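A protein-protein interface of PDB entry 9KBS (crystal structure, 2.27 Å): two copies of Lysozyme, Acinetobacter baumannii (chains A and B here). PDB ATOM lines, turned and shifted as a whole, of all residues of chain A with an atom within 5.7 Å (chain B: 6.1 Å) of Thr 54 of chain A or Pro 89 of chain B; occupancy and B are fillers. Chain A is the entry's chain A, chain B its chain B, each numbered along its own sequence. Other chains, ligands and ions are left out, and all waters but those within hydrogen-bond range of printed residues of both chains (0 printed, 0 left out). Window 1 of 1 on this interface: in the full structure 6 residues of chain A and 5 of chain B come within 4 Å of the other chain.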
ATOM      1  N   SER A  49     -15.712  25.983  12.769  1.00  0.00           N
ATOM      2  CA  SER A  49     -15.516  24.545  12.615  1.00  0.00           C
ATOM      3  C   SER A  49     -14.853  24.209  11.285  1.00  0.00           C
ATOM      4  O   SER A  49     -13.960  23.356  11.228  1.00  0.00           O
ATOM      5  CB  SER A  49     -16.860  23.828  12.737  1.00  0.00           C
ATOM      6  OG  SER A  49     -17.185  23.593  14.094  1.00  0.00           O
ATOM      7  N   GLU A  52     -11.136  25.330  11.542  1.00  0.00           N
ATOM      8  CA  GLU A  52     -10.373  24.599  12.545  1.00  0.00           C
ATOM      9  C   GLU A  52     -10.205  23.128  12.188  1.00  0.00           C
ATOM     10  O   GLU A  52      -9.175  22.529  12.519  1.00  0.00           O
ATOM     11  CB  GLU A  52     -11.053  24.709  13.914  1.00  0.00           C
ATOM     12  CG  GLU A  52     -11.140  26.118  14.484  1.00  0.00           C
ATOM     13  CD  GLU A  52      -9.797  26.655  14.927  1.00  0.00           C
ATOM     14  OE1 GLU A  52      -8.899  25.840  15.222  1.00  0.00           O
ATOM     15  OE2 GLU A  52      -9.644  27.893  14.988  1.00  0.00           O
ATOM     16  N   GLY A  53     -11.190  22.532  11.522  1.00  0.00           N
ATOM     17  CA  GLY A  53     -11.242  21.090  11.388  1.00  0.00           C
ATOM     18  C   GLY A  53     -11.544  20.416  12.711  1.00  0.00           C
ATOM     19  O   GLY A  53     -11.516  21.060  13.765  1.00  0.00           O
ATOM     20  N   THR A  54     -11.844  19.120  12.677  1.00  0.00           N
ATOM     21  CA  THR A  54     -12.043  18.338  13.888  1.00  0.00           C
ATOM     22  C   THR A  54     -11.179  17.088  13.830  1.00  0.00           C
ATOM     23  O   THR A  54     -11.131  16.412  12.799  1.00  0.00           O
ATOM     24  CB  THR A  54     -13.519  17.957  14.067  1.00  0.00           C
ATOM     25  OG1 THR A  54     -14.296  19.144  14.260  1.00  0.00           O
ATOM     26  CG2 THR A  54     -13.699  17.051  15.277  1.00  0.00           C
ATOM     27  N   ARG A  55     -10.427  16.825  14.894  1.00  0.00           N
ATOM     28  CA  ARG A  55      -9.629  15.614  15.006  1.00  0.00           C
ATOM     29  C   ARG A  55      -9.754  15.083  16.437  1.00  0.00           C
ATOM     30  O   ARG A  55      -9.948  15.832  17.349  1.00  0.00           O
ATOM     31  CB  ARG A  55      -8.191  15.815  14.565  1.00  0.00           C
ATOM     32  CG  ARG A  55      -7.663  14.705  13.683  1.00  0.00           C
ATOM     33  CD  ARG A  55      -6.815  13.789  14.536  1.00  0.00           C
ATOM     34  NE  ARG A  55      -6.681  12.398  14.107  1.00  0.00           N
ATOM     35  CZ  ARG A  55      -7.601  11.443  14.229  1.00  0.00           C
ATOM     36  NH1 ARG A  55      -8.810  11.698  14.696  1.00  0.00           N
ATOM     37  NH2 ARG A  55      -7.319  10.222  13.808  1.00  0.00           N
ATOM     38  N   PHE A  56      -9.659  13.783  16.626  1.00  0.00           N
ATOM     39  CA  PHE A  56      -9.865  13.156  17.925  1.00  0.00           C
ATOM     40  C   PHE A  56      -8.582  12.572  18.500  1.00  0.00           C
ATOM     41  O   PHE A  56      -8.626  11.889  19.528  1.00  0.00           O
ATOM     42  CB  PHE A  56     -10.957  12.088  17.823  1.00  0.00           C
ATOM     43  CG  PHE A  56     -12.311  12.652  17.477  1.00  0.00           C
ATOM     44  CD1 PHE A  56     -12.734  13.848  18.032  1.00  0.00           C
ATOM     45  CD2 PHE A  56     -13.147  12.001  16.584  1.00  0.00           C
ATOM     46  CE1 PHE A  56     -13.968  14.381  17.714  1.00  0.00           C
ATOM     47  CE2 PHE A  56     -14.384  12.531  16.260  1.00  0.00           C
ATOM     48  CZ  PHE A  56     -14.795  13.723  16.826  1.00  0.00           C
ATOM     49  N   GLY A  69      -9.729  17.964  19.035  1.00  0.00           N
ATOM     50  CA  GLY A  69     -11.110  18.368  18.833  1.00  0.00           C
ATOM     51  C   GLY A  69     -11.222  19.388  17.721  1.00  0.00           C
ATOM     52  O   GLY A  69     -10.561  19.288  16.681  1.00  0.00           O
ATOM     53  N   THR A  70     -12.073  20.390  17.936  1.00  0.00           N
ATOM     54  CA  THR A  70     -12.256  21.471  16.969  1.00  0.00           C
ATOM     55  C   THR A  70     -11.444  22.691  17.408  1.00  0.00           C
ATOM     56  O   THR A  70     -11.968  23.704  17.875  1.00  0.00           O
ATOM     57  CB  THR A  70     -13.738  21.800  16.810  1.00  0.00           C
ATOM     58  OG1 THR A  70     -14.475  20.587  16.608  1.00  0.00           O
ATOM     59  CG2 THR A  70     -13.957  22.719  15.609  1.00  0.00           C
ATOM     60  N   ALA A  92     -14.984  16.634  22.477  1.00  0.00           N
ATOM     61  CA  ALA A  92     -14.636  17.739  21.589  1.00  0.00           C
ATOM     62  C   ALA A  92     -15.748  18.780  21.547  1.00  0.00           C
ATOM     63  O   ALA A  92     -15.478  19.986  21.540  1.00  0.00           O
ATOM     64  CB  ALA A  92     -14.333  17.210  20.187  1.00  0.00           C
ATOM     65  N   PHE B  56     -20.441  12.843  13.704  1.00  0.00           N
ATOM     66  CA  PHE B  56     -19.707  11.595  13.850  1.00  0.00           C
ATOM     67  C   PHE B  56     -20.534  10.477  14.475  1.00  0.00           C
ATOM     68  O   PHE B  56     -19.993   9.401  14.755  1.00  0.00           O
ATOM     69  CB  PHE B  56     -18.433  11.854  14.654  1.00  0.00           C
ATOM     70  CG  PHE B  56     -17.590  12.959  14.079  1.00  0.00           C
ATOM     71  CD1 PHE B  56     -16.847  12.750  12.930  1.00  0.00           C
ATOM     72  CD2 PHE B  56     -17.582  14.217  14.658  1.00  0.00           C
ATOM     73  CE1 PHE B  56     -16.087  13.769  12.384  1.00  0.00           C
ATOM     74  CE2 PHE B  56     -16.826  15.241  14.115  1.00  0.00           C
ATOM     75  CZ  PHE B  56     -16.076  15.016  12.977  1.00  0.00           C
ATOM     76  N   CYS B  87     -18.255   7.273  13.090  1.00  0.00           N
ATOM     77  CA  CYS B  87     -17.125   7.423  12.185  1.00  0.00           C
ATOM     78  C   CYS B  87     -16.151   8.445  12.756  1.00  0.00           C
ATOM     79  O   CYS B  87     -16.473   9.203  13.675  1.00  0.00           O
ATOM     80  CB  CYS B  87     -17.577   7.831  10.776  1.00  0.00           C
ATOM     81  SG  CYS B  87     -18.159   9.534  10.618  1.00  0.00           S
ATOM     82  N   THR B  88     -14.948   8.456  12.190  1.00  0.00           N
ATOM     83  CA  THR B  88     -13.894   9.400  12.515  1.00  0.00           C
ATOM     84  C   THR B  88     -13.862  10.532  11.498  1.00  0.00           C
ATOM     85  O   THR B  88     -14.455  10.429  10.420  1.00  0.00           O
ATOM     86  CB  THR B  88     -12.536   8.686  12.546  1.00  0.00           C
ATOM     87  OG1 THR B  88     -12.161   8.317  11.214  1.00  0.00           O
ATOM     88  CG2 THR B  88     -12.601   7.433  13.423  1.00  0.00           C
ATOM     89  N   PRO B  89     -13.198  11.650  11.818  1.00  0.00           N
ATOM     90  CA  PRO B  89     -13.047  12.721  10.816  1.00  0.00           C
ATOM     91  C   PRO B  89     -12.447  12.254   9.499  1.00  0.00           C
ATOM     92  O   PRO B  89     -12.940  12.642   8.432  1.00  0.00           O
ATOM     93  CB  PRO B  89     -12.146  13.734  11.535  1.00  0.00           C
ATOM     94  CG  PRO B  89     -12.448  13.529  12.973  1.00  0.00           C
ATOM     95  CD  PRO B  89     -12.653  12.051  13.129  1.00  0.00           C
ATOM     96  N   GLU B  90     -11.393  11.435   9.542  1.00  0.00           N
ATOM     97  CA  GLU B  90     -10.778  10.957   8.306  1.00  0.00           C
ATOM     98  C   GLU B  90     -11.749  10.108   7.494  1.00  0.00           C
ATOM     99  O   GLU B  90     -11.792  10.202   6.259  1.00  0.00           O
ATOM    100  CB  GLU B  90      -9.514  10.154   8.627  1.00  0.00           C
ATOM    101  CG  GLU B  90      -8.409  10.961   9.289  1.00  0.00           C
ATOM    102  CD  GLU B  90      -8.616  11.169  10.779  1.00  0.00           C
ATOM    103  OE1 GLU B  90      -9.529  10.548  11.362  1.00  0.00           O
ATOM    104  OE2 GLU B  90      -7.877  11.987  11.360  1.00  0.00           O
ATOM    105  N   GLN B  91     -12.550   9.284   8.168  1.00  0.00           N
ATOM    106  CA  GLN B  91     -13.518   8.459   7.455  1.00  0.00           C
ATOM    107  C   GLN B  91     -14.605   9.316   6.818  1.00  0.00           C
ATOM    108  O   GLN B  91     -15.020   9.062   5.680  1.00  0.00           O
ATOM    109  CB  GLN B  91     -14.113   7.419   8.401  1.00  0.00           C
ATOM    110  CG  GLN B  91     -13.121   6.333   8.799  1.00  0.00           C
ATOM    111  CD  GLN B  91     -13.550   5.574  10.038  1.00  0.00           C
ATOM    112  OE1 GLN B  91     -14.637   5.797  10.570  1.00  0.00           O
ATOM    113  NE2 GLN B  91     -12.694   4.672  10.507  1.00  0.00           N
ATOM    114  N   ALA B  92     -15.107  10.311   7.556  1.00  0.00           N
ATOM    115  CA  ALA B  92     -16.070  11.242   6.980  1.00  0.00           C
ATOM    116  C   ALA B  92     -15.494  11.945   5.758  1.00  0.00           C
ATOM    117  O   ALA B  92     -16.186  12.117   4.749  1.00  0.00           O
ATOM    118  CB  ALA B  92     -16.508  12.260   8.034  1.00  0.00           C
ATOM    119  N   LYS B  93     -14.220  12.348   5.829  1.00  0.00           N
ATOM    120  CA  LYS B  93     -13.565  12.956   4.674  1.00  0.00           C
ATOM    121  C   LYS B  93     -13.535  12.002   3.487  1.00  0.00           C
ATOM    122  O   LYS B  93     -13.815  12.405   2.350  1.00  0.00           O
ATOM    123  CB  LYS B  93     -12.148  13.396   5.045  1.00  0.00           C
ATOM    124  CG  LYS B  93     -11.405  14.109   3.924  1.00  0.00           C
ATOM    125  CD  LYS B  93     -10.019  14.569   4.361  1.00  0.00           C
ATOM    126  CE  LYS B  93      -9.275  15.259   3.224  1.00  0.00           C
ATOM    127  NZ  LYS B  93      -7.916  15.716   3.636  1.00  0.00           N
ATOM    128  N   SER B  94     -13.190  10.734   3.727  1.00  0.00           N
ATOM    129  CA  SER B  94     -13.124   9.773   2.629  1.00  0.00           C
ATOM    130  C   SER B  94     -14.494   9.565   1.992  1.00  0.00           C
ATOM    131  O   SER B  94     -14.622   9.530   0.759  1.00  0.00           O
ATOM    132  CB  SER B  94     -12.563   8.444   3.130  1.00  0.00           C
ATOM    133  OG  SER B  94     -11.221   8.586   3.560  1.00  0.00           O
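Phe 56 of chain B touches its own counterpart, Phe 56 of chain A. Positions printed for both chains: 56 and 92.
Printed residues of chain B that touch a printed residue of chain A: Phe 56, Pro 89 and Glu 90. Along chain B the printed residues that touch a printed residue of chain A span positions 56 to 90. Of the 9 printed residues of chain A, 3 touch a printed residue of chain B. Printed residues of chain A that touch a printed residue of chain B: Thr 54, Arg 55 and Phe 56.
The guanidinium group of Arg 55 of chain A is in salt-bridge range of the side-chain carboxylate of Glu 90 of chain B, at 3.0 Å.
The backbone carbonyl oxygen (O) of Glu 90 of chain B sits at hydrogen-bond distance from the side-chain hydroxyl (OG) of Ser 94 of chain B. OG1 of Thr 70 of chain A is in hydrogen-bond range of OG1 of Thr 54 of chain A (2.8 Å). N of Cys 87 of chain B lies within hydrogen-bond range of O of Phe 56 of chain B, at 3.2 Å. The backbone NH (N) of Gly 69 of chain A sits at hydrogen-bond distance from the backbone carbonyl oxygen (O) of Arg 55 of chain A, at 2.7 Å. The side-chain carboxylate (OE1) of Glu 90 of chain B lies within hydrogen-bond range of the side-chain hydroxyl (OG1) of Thr 88 of chain B, 3.5 Å away.
Of chain B, only Phe 56 and Pro 89 come within 4 Å of Thr 54 of chain A. Of the printed residues of chain B, Arg 55 of chain A touches Glu 90 (2.9 Å). Printed residues of chain B within 4 Å of Phe 56 of chain A: Phe 56 and Pro 89. Of the printed residues of chain A, Phe 56 of chain B touches Thr 54 and Phe 56. Pro 89 of chain B touches just these residues of chain A: Thr 54 and Phe 56. Of the printed residues of chain A, Glu 90 of chain B touches Arg 55. The nearest residue of chain A that does not touch Pro 89 of chain B is Arg 55 of chain A (4.1 Å).
Among the printed residues, merely in contact across the chains: Thr 54 of chain A with Pro 89 of chain B (3.1 Å), Phe 56 of chain A with Pro 89 of chain B (3.5 Å), Phe 56 of chain A with Phe 56 of chain B (3.6 Å) and Thr 54 of chain A with Phe 56 of chain B (3.8 Å).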
